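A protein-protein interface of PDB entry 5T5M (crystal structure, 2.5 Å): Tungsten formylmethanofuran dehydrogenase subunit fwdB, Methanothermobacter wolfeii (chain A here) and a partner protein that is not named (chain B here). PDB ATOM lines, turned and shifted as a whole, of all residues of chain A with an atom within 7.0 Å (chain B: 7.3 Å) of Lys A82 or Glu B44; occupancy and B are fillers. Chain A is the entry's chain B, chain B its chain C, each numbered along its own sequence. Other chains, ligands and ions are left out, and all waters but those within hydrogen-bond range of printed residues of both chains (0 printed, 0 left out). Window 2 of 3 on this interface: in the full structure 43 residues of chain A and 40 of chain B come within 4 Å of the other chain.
The side-chain amide nitrogen of Asn B43 is in hydrogen-bond range of the backbone carbonyl oxygen of Ser A81. The backbone NH (N) of Asn B43 is in hydrogen-bond range of the backbone carbonyl oxygen (O) of Lys A82 (2.9 Å). The backbone carbonyl oxygen (O) of Ala A107 lies within hydrogen-bond range of the side-chain amide nitrogen (ND2) of Asn B43 (3.1 Å).
The backbone carbonyl oxygen of Ile A77 lies within hydrogen-bond range of the side-chain hydroxyl of Ser A81, at 3.1 Å. The backbone NH (N) of Lys A82 is in hydrogen-bond range of the side-chain carboxylate (OD2) of Asp A336, 3.1 Å away. OE1 of Glu A334 is in salt-bridge range of NE of Arg A83 (3.0 Å). The backbone carbonyl oxygen (O) of Arg A83 lies within hydrogen-bond range of the backbone NH (N) of Asp A336, 3.3 Å away. ND1 of His B41 lies within hydrogen-bond range of O of Val B14 (3.3 Å). O of Glu B17 is in hydrogen-bond range of N of Met B40.
Gly B42 touches Lys A82 (CA to O, 3.1 Å). Lys A82 touches Glu B44 (CE to OE1, 3.4 Å). Arg A83 touches Val B14 (CB to CG1, 3.8 Å). Pro A84 touches Asn B43 (CD to ND2, 3.8 Å). Gly A108 touches Asn B43. Met B40 touches Ser A313. Ser A313 touches Gly B42. O of Ser A313 touches CA of Asn B43, 3.6 Å away. CG of Pro B15 touches CD of Glu A334 (3.5 Å). Val B14 touches Asp A336 (CG2 to OD2, 3.7 Å).
Lys A82 touches just these residues of chain B: His B41, Gly B42, Asn B43 and Glu B44. Printed residues of chain A within 4 Å of Met B40: Ser A313 (3.9 Å). Of the printed residues of chain A, Asn B43 touches Ser A81, Lys A82, Pro A84, Ala A107, Gly A108 and Ser A313. Glu B44 touches just one residue of chain A: Lys A82 (3.4 Å). The nearest residue of chain A that does not touch Glu B44 is Ser A313 (5.0 Å).
Hydrophobic or aromatic side chains of chain B within 4 Å of the printed part of chain A: Val B14, Pro B15, Met B40 and His B41. Of the 15 printed residues of chain A, 9 touch a printed residue of chain B.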
ATOM      1  N   ILE A  77      -1.969 -24.895   5.322  1.00  0.00           N
ATOM      2  CA  ILE A  77      -0.559 -25.054   4.979  1.00  0.00           C
ATOM      3  C   ILE A  77      -0.396 -26.050   3.839  1.00  0.00           C
ATOM      4  O   ILE A  77       0.312 -25.789   2.860  1.00  0.00           O
ATOM      5  CB  ILE A  77       0.247 -25.477   6.221  1.00  0.00           C
ATOM      6  CG1 ILE A  77       0.285 -24.316   7.227  1.00  0.00           C
ATOM      7  CG2 ILE A  77       1.657 -25.939   5.823  1.00  0.00           C
ATOM      8  CD1 ILE A  77       1.038 -24.601   8.496  1.00  0.00           C
ATOM      9  N   LEU A  78      -1.047 -27.211   3.949  1.00  0.00           N
ATOM     10  CA  LEU A  78      -0.839 -28.270   2.965  1.00  0.00           C
ATOM     11  C   LEU A  78      -1.396 -27.882   1.605  1.00  0.00           C
ATOM     12  O   LEU A  78      -0.810 -28.224   0.568  1.00  0.00           O
ATOM     13  CB  LEU A  78      -1.493 -29.561   3.446  1.00  0.00           C
ATOM     14  CG  LEU A  78      -0.981 -30.091   4.781  1.00  0.00           C
ATOM     15  CD1 LEU A  78      -1.835 -31.266   5.270  1.00  0.00           C
ATOM     16  CD2 LEU A  78       0.482 -30.494   4.642  1.00  0.00           C
ATOM     17  N   ALA A  79      -2.522 -27.166   1.589  1.00  0.00           N
ATOM     18  CA  ALA A  79      -3.237 -26.897   0.348  1.00  0.00           C
ATOM     19  C   ALA A  79      -2.548 -25.843  -0.506  1.00  0.00           C
ATOM     20  O   ALA A  79      -2.773 -25.807  -1.720  1.00  0.00           O
ATOM     21  CB  ALA A  79      -4.673 -26.453   0.654  1.00  0.00           C
ATOM     22  N   GLU A  80      -1.727 -24.985   0.091  1.00  0.00           N
ATOM     23  CA  GLU A  80      -1.002 -23.982  -0.670  1.00  0.00           C
ATOM     24  C   GLU A  80       0.462 -24.339  -0.871  1.00  0.00           C
ATOM     25  O   GLU A  80       1.185 -23.579  -1.523  1.00  0.00           O
ATOM     26  CB  GLU A  80      -1.127 -22.614   0.009  1.00  0.00           C
ATOM     27  CG  GLU A  80      -0.540 -22.528   1.401  1.00  0.00           C
ATOM     28  CD  GLU A  80      -1.027 -21.296   2.145  1.00  0.00           C
ATOM     29  OE1 GLU A  80      -2.233 -20.982   2.049  1.00  0.00           O
ATOM     30  OE2 GLU A  80      -0.202 -20.636   2.811  1.00  0.00           O
ATOM     31  N   SER A  81       0.907 -25.484  -0.359  1.00  0.00           N
ATOM     32  CA  SER A  81       2.255 -25.951  -0.641  1.00  0.00           C
ATOM     33  C   SER A  81       2.360 -26.458  -2.071  1.00  0.00           C
ATOM     34  O   SER A  81       1.376 -26.889  -2.678  1.00  0.00           O
ATOM     35  CB  SER A  81       2.656 -27.070   0.316  1.00  0.00           C
ATOM     36  OG  SER A  81       3.016 -26.547   1.577  1.00  0.00           O
ATOM     37  N   LYS A  82       3.574 -26.392  -2.608  1.00  0.00           N
ATOM     38  CA  LYS A  82       3.877 -26.933  -3.921  1.00  0.00           C
ATOM     39  C   LYS A  82       4.683 -28.217  -3.856  1.00  0.00           C
ATOM     40  O   LYS A  82       4.817 -28.897  -4.877  1.00  0.00           O
ATOM     41  CB  LYS A  82       4.629 -25.885  -4.756  1.00  0.00           C
ATOM     42  CG  LYS A  82       3.687 -24.902  -5.406  1.00  0.00           C
ATOM     43  CD  LYS A  82       4.355 -23.604  -5.761  1.00  0.00           C
ATOM     44  CE  LYS A  82       3.328 -22.623  -6.305  1.00  0.00           C
ATOM     45  NZ  LYS A  82       3.820 -21.222  -6.296  1.00  0.00           N
ATOM     46  N   ARG A  83       5.209 -28.567  -2.682  1.00  0.00           N
ATOM     47  CA  ARG A  83       5.939 -29.817  -2.487  1.00  0.00           C
ATOM     48  C   ARG A  83       5.826 -30.214  -1.023  1.00  0.00           C
ATOM     49  O   ARG A  83       6.806 -30.186  -0.274  1.00  0.00           O
ATOM     50  CB  ARG A  83       7.394 -29.656  -2.895  1.00  0.00           C
ATOM     51  CG  ARG A  83       8.108 -30.962  -3.061  1.00  0.00           C
ATOM     52  CD  ARG A  83       8.183 -31.322  -4.518  1.00  0.00           C
ATOM     53  NE  ARG A  83       9.122 -32.415  -4.768  1.00  0.00           N
ATOM     54  CZ  ARG A  83       8.797 -33.584  -5.310  1.00  0.00           C
ATOM     55  NH1 ARG A  83       7.543 -33.844  -5.670  1.00  0.00           N
ATOM     56  NH2 ARG A  83       9.743 -34.505  -5.497  1.00  0.00           N
ATOM     57  N   PRO A  84       4.628 -30.576  -0.572  1.00  0.00           N
ATOM     58  CA  PRO A  84       4.457 -30.934   0.841  1.00  0.00           C
ATOM     59  C   PRO A  84       4.794 -32.390   1.131  1.00  0.00           C
ATOM     60  O   PRO A  84       4.485 -33.300   0.360  1.00  0.00           O
ATOM     61  CB  PRO A  84       2.970 -30.652   1.079  1.00  0.00           C
ATOM     62  CG  PRO A  84       2.340 -30.924  -0.247  1.00  0.00           C
ATOM     63  CD  PRO A  84       3.341 -30.532  -1.292  1.00  0.00           C
ATOM     64  N   ALA A 107      -3.513 -33.388  -1.939  1.00  0.00           N
ATOM     65  CA  ALA A 107      -2.576 -32.299  -1.704  1.00  0.00           C
ATOM     66  C   ALA A 107      -1.423 -32.275  -2.699  1.00  0.00           C
ATOM     67  O   ALA A 107      -0.645 -31.315  -2.691  1.00  0.00           O
ATOM     68  CB  ALA A 107      -2.018 -32.398  -0.282  1.00  0.00           C
ATOM     69  N   GLY A 108      -1.295 -33.284  -3.555  1.00  0.00           N
ATOM     70  CA  GLY A 108      -0.144 -33.361  -4.432  1.00  0.00           C
ATOM     71  C   GLY A 108       1.134 -33.615  -3.675  1.00  0.00           C
ATOM     72  O   GLY A 108       2.198 -33.163  -4.093  1.00  0.00           O
ATOM     73  N   ALA A 109       1.053 -34.343  -2.570  1.00  0.00           N
ATOM     74  CA  ALA A 109       2.161 -34.467  -1.652  1.00  0.00           C
ATOM     75  C   ALA A 109       3.066 -35.633  -2.031  1.00  0.00           C
ATOM     76  O   ALA A 109       2.772 -36.438  -2.918  1.00  0.00           O
ATOM     77  CB  ALA A 109       1.644 -34.651  -0.226  1.00  0.00           C
ATOM     78  N   SER A 313       2.640 -35.556  -7.087  1.00  0.00           N
ATOM     79  CA  SER A 313       2.673 -34.210  -7.647  1.00  0.00           C
ATOM     80  C   SER A 313       2.099 -34.162  -9.053  1.00  0.00           C
ATOM     81  O   SER A 313       1.519 -33.146  -9.447  1.00  0.00           O
ATOM     82  CB  SER A 313       4.110 -33.690  -7.656  1.00  0.00           C
ATOM     83  OG  SER A 313       4.934 -34.511  -8.474  1.00  0.00           O
ATOM     84  N   GLU A 334      13.824 -29.424  -1.060  1.00  0.00           N
ATOM     85  CA  GLU A 334      12.683 -29.453  -1.972  1.00  0.00           C
ATOM     86  C   GLU A 334      11.367 -29.168  -1.250  1.00  0.00           C
ATOM     87  O   GLU A 334      10.495 -28.487  -1.799  1.00  0.00           O
ATOM     88  CB  GLU A 334      12.592 -30.814  -2.676  1.00  0.00           C
ATOM     89  CG  GLU A 334      13.741 -31.159  -3.609  1.00  0.00           C
ATOM     90  CD  GLU A 334      13.370 -32.251  -4.624  1.00  0.00           C
ATOM     91  OE1 GLU A 334      12.158 -32.523  -4.815  1.00  0.00           O
ATOM     92  OE2 GLU A 334      14.296 -32.834  -5.233  1.00  0.00           O
ATOM     93  N   ASP A 336       8.505 -27.681   1.144  1.00  0.00           N
ATOM     94  CA  ASP A 336       8.141 -26.412   1.755  1.00  0.00           C
ATOM     95  C   ASP A 336       7.146 -26.566   2.899  1.00  0.00           C
ATOM     96  O   ASP A 336       6.756 -25.561   3.499  1.00  0.00           O
ATOM     97  CB  ASP A 336       7.569 -25.457   0.697  1.00  0.00           C
ATOM     98  CG  ASP A 336       6.496 -26.097  -0.141  1.00  0.00           C
ATOM     99  OD1 ASP A 336       5.981 -27.160   0.259  1.00  0.00           O
ATOM    100  OD2 ASP A 336       6.160 -25.531  -1.198  1.00  0.00           O
ATOM    101  N   ALA A 337       6.725 -27.789   3.216  1.00  0.00           N
ATOM    102  CA  ALA A 337       5.909 -28.035   4.397  1.00  0.00           C
ATOM    103  C   ALA A 337       6.037 -29.504   4.767  1.00  0.00           C
ATOM    104  O   ALA A 337       6.141 -30.358   3.884  1.00  0.00           O
ATOM    105  CB  ALA A 337       4.436 -27.668   4.162  1.00  0.00           C
ATOM    106  N   VAL B  14      11.601 -25.226  -4.822  1.00  0.00           N
ATOM    107  CA  VAL B  14      10.823 -26.387  -5.260  1.00  0.00           C
ATOM    108  C   VAL B  14      11.207 -26.684  -6.709  1.00  0.00           C
ATOM    109  O   VAL B  14      10.878 -25.888  -7.602  1.00  0.00           O
ATOM    110  CB  VAL B  14       9.311 -26.144  -5.119  1.00  0.00           C
ATOM    111  CG1 VAL B  14       8.516 -27.297  -5.722  1.00  0.00           C
ATOM    112  CG2 VAL B  14       8.937 -25.969  -3.647  1.00  0.00           C
ATOM    113  N   PRO B  15      11.889 -27.796  -6.993  1.00  0.00           N
ATOM    114  CA  PRO B  15      12.491 -27.974  -8.320  1.00  0.00           C
ATOM    115  C   PRO B  15      11.476 -28.032  -9.450  1.00  0.00           C
ATOM    116  O   PRO B  15      10.278 -28.250  -9.254  1.00  0.00           O
ATOM    117  CB  PRO B  15      13.239 -29.311  -8.193  1.00  0.00           C
ATOM    118  CG  PRO B  15      13.498 -29.461  -6.752  1.00  0.00           C
ATOM    119  CD  PRO B  15      12.283 -28.881  -6.080  1.00  0.00           C
ATOM    120  N   LEU B  16      11.996 -27.838 -10.660  1.00  0.00           N
ATOM    121  CA  LEU B  16      11.238 -27.993 -11.890  1.00  0.00           C
ATOM    122  C   LEU B  16      11.486 -29.370 -12.493  1.00  0.00           C
ATOM    123  O   LEU B  16      12.579 -29.929 -12.379  1.00  0.00           O
ATOM    124  CB  LEU B  16      11.627 -26.917 -12.907  1.00  0.00           C
ATOM    125  CG  LEU B  16      11.438 -25.461 -12.484  1.00  0.00           C
ATOM    126  CD1 LEU B  16      11.871 -24.541 -13.619  1.00  0.00           C
ATOM    127  CD2 LEU B  16       9.983 -25.166 -12.058  1.00  0.00           C
ATOM    128  N   GLU B  17      10.455 -29.922 -13.128  1.00  0.00           N
ATOM    129  CA  GLU B  17      10.606 -31.058 -14.029  1.00  0.00           C
ATOM    130  C   GLU B  17      10.219 -30.576 -15.415  1.00  0.00           C
ATOM    131  O   GLU B  17       9.107 -30.077 -15.612  1.00  0.00           O
ATOM    132  CB  GLU B  17       9.739 -32.249 -13.618  1.00  0.00           C
ATOM    133  CG  GLU B  17       9.994 -32.769 -12.222  1.00  0.00           C
ATOM    134  CD  GLU B  17       9.180 -34.007 -11.904  1.00  0.00           C
ATOM    135  OE1 GLU B  17       8.871 -34.204 -10.710  1.00  0.00           O
ATOM    136  OE2 GLU B  17       8.846 -34.775 -12.841  1.00  0.00           O
ATOM    137  N   ILE B  39       5.806 -27.317 -18.181  1.00  0.00           N
ATOM    138  CA  ILE B  39       6.756 -27.924 -17.259  1.00  0.00           C
ATOM    139  C   ILE B  39       6.070 -28.032 -15.902  1.00  0.00           C
ATOM    140  O   ILE B  39       5.044 -27.398 -15.647  1.00  0.00           O
ATOM    141  CB  ILE B  39       8.080 -27.124 -17.153  1.00  0.00           C
ATOM    142  CG1 ILE B  39       7.846 -25.767 -16.479  1.00  0.00           C
ATOM    143  CG2 ILE B  39       8.688 -26.940 -18.541  1.00  0.00           C
ATOM    144  CD1 ILE B  39       9.103 -24.923 -16.322  1.00  0.00           C
ATOM    145  N   MET B  40       6.642 -28.849 -15.025  1.00  0.00           N
ATOM    146  CA  MET B  40       6.124 -28.994 -13.673  1.00  0.00           C
ATOM    147  C   MET B  40       6.897 -28.097 -12.715  1.00  0.00           C
ATOM    148  O   MET B  40       8.120 -27.958 -12.822  1.00  0.00           O
ATOM    149  CB  MET B  40       6.210 -30.440 -13.188  1.00  0.00           C
ATOM    150  CG  MET B  40       5.409 -31.447 -13.996  1.00  0.00           C
ATOM    151  SD  MET B  40       3.653 -31.045 -14.087  1.00  0.00           S
ATOM    152  CE  MET B  40       3.108 -31.203 -12.383  1.00  0.00           C
ATOM    153  N   HIS B  41       6.164 -27.479 -11.789  1.00  0.00           N
ATOM    154  CA  HIS B  41       6.726 -26.740 -10.658  1.00  0.00           C
ATOM    155  C   HIS B  41       6.050 -27.300  -9.408  1.00  0.00           C
ATOM    156  O   HIS B  41       5.004 -26.813  -8.967  1.00  0.00           O
ATOM    157  CB  HIS B  41       6.508 -25.229 -10.807  1.00  0.00           C
ATOM    158  CG  HIS B  41       6.955 -24.440  -9.618  1.00  0.00           C
ATOM    159  ND1 HIS B  41       8.213 -24.572  -9.069  1.00  0.00           N
ATOM    160  CD2 HIS B  41       6.311 -23.520  -8.863  1.00  0.00           C
ATOM    161  CE1 HIS B  41       8.327 -23.761  -8.033  1.00  0.00           C
ATOM    162  NE2 HIS B  41       7.188 -23.111  -7.885  1.00  0.00           N
ATOM    163  N   GLY B  42       6.650 -28.336  -8.832  1.00  0.00           N
ATOM    164  CA  GLY B  42       5.983 -29.039  -7.752  1.00  0.00           C
ATOM    165  C   GLY B  42       4.706 -29.663  -8.262  1.00  0.00           C
ATOM    166  O   GLY B  42       4.652 -30.195  -9.375  1.00  0.00           O
ATOM    167  N   ASN B  43       3.652 -29.579  -7.452  1.00  0.00           N
ATOM    168  CA  ASN B  43       2.325 -30.053  -7.834  1.00  0.00           C
ATOM    169  C   ASN B  43       1.569 -29.058  -8.713  1.00  0.00           C
ATOM    170  O   ASN B  43       0.337 -29.111  -8.750  1.00  0.00           O
ATOM    171  CB  ASN B  43       1.497 -30.372  -6.585  1.00  0.00           C
ATOM    172  CG  ASN B  43       1.428 -29.206  -5.625  1.00  0.00           C
ATOM    173  OD1 ASN B  43       1.526 -28.048  -6.035  1.00  0.00           O
ATOM    174  ND2 ASN B  43       1.271 -29.505  -4.335  1.00  0.00           N
ATOM    175  N   GLU B  44       2.262 -28.161  -9.410  1.00  0.00           N
ATOM    176  CA  GLU B  44       1.642 -27.196 -10.306  1.00  0.00           C
ATOM    177  C   GLU B  44       2.244 -27.341 -11.693  1.00  0.00           C
ATOM    178  O   GLU B  44       3.465 -27.461 -11.832  1.00  0.00           O
ATOM    179  CB  GLU B  44       1.850 -25.761  -9.811  1.00  0.00           C
ATOM    180  CG  GLU B  44       0.844 -25.296  -8.775  1.00  0.00           C
ATOM    181  CD  GLU B  44       0.840 -23.778  -8.606  1.00  0.00           C
ATOM    182  OE1 GLU B  44       1.690 -23.103  -9.231  1.00  0.00           O
ATOM    183  OE2 GLU B  44      -0.015 -23.260  -7.852  1.00  0.00           O
ATOM    184  N   VAL B  45       1.392 -27.339 -12.713  1.00  0.00           N
ATOM    185  CA  VAL B  45       1.844 -27.215 -14.094  1.00  0.00           C
ATOM    186  C   VAL B  45       1.999 -25.735 -14.403  1.00  0.00           C
ATOM    187  O   VAL B  45       1.105 -24.932 -14.116  1.00  0.00           O
ATOM    188  CB  VAL B  45       0.859 -27.880 -15.074  1.00  0.00           C
ATOM    189  CG1 VAL B  45       1.372 -27.740 -16.512  1.00  0.00           C
ATOM    190  CG2 VAL B  45       0.638 -29.353 -14.727  1.00  0.00           C
ATOM    191  N   VAL B  46       3.137 -25.370 -14.978  1.00  0.00           N
ATOM    192  CA  VAL B  46       3.420 -23.989 -15.327  1.00  0.00           C
ATOM    193  C   VAL B  46       3.954 -23.953 -16.749  1.00  0.00           C
ATOM    194  O   VAL B  46       4.218 -24.983 -17.368  1.00  0.00           O
ATOM    195  CB  VAL B  46       4.419 -23.336 -14.347  1.00  0.00           C
ATOM    196  CG1 VAL B  46       3.796 -23.231 -12.955  1.00  0.00           C
ATOM    197  CG2 VAL B  46       5.719 -24.136 -14.292  1.00  0.00           C
ATOM    198  N   LYS B  47       4.114 -22.746 -17.262  1.00  0.00           N
ATOM    199  CA  LYS B  47       4.635 -22.562 -18.605  1.00  0.00           C
ATOM    200  C   LYS B  47       6.146 -22.374 -18.556  1.00  0.00           C
ATOM    201  O   LYS B  47       6.697 -21.839 -17.590  1.00  0.00           O
ATOM    202  CB  LYS B  47       3.963 -21.363 -19.271  1.00  0.00           C
ATOM    203  CG  LYS B  47       2.457 -21.540 -19.448  1.00  0.00           C
ATOM    204  CD  LYS B  47       1.795 -20.327 -20.058  1.00  0.00           C
ATOM    205  CE  LYS B  47       1.793 -19.149 -19.097  1.00  0.00           C
ATOM    206  NZ  LYS B  47       1.176 -17.926 -19.707  1.00  0.00           N
ATOM    207  N   PHE B  51       9.706 -19.410 -16.196  1.00  0.00           N
ATOM    208  CA  PHE B  51      11.023 -19.577 -15.608  1.00  0.00           C
ATOM    209  C   PHE B  51      12.162 -19.422 -16.611  1.00  0.00           C
ATOM    210  O   PHE B  51      13.330 -19.510 -16.215  1.00  0.00           O
ATOM    211  CB  PHE B  51      11.115 -20.951 -14.917  1.00  0.00           C
ATOM    212  CG  PHE B  51      10.258 -21.058 -13.694  1.00  0.00           C
ATOM    213  CD1 PHE B  51       8.932 -21.437 -13.793  1.00  0.00           C
ATOM    214  CD2 PHE B  51      10.772 -20.760 -12.445  1.00  0.00           C
ATOM    215  CE1 PHE B  51       8.131 -21.526 -12.664  1.00  0.00           C
ATOM    216  CE2 PHE B  51       9.983 -20.845 -11.314  1.00  0.00           C
ATOM    217  CZ  PHE B  51       8.655 -21.233 -11.424  1.00  0.00           C
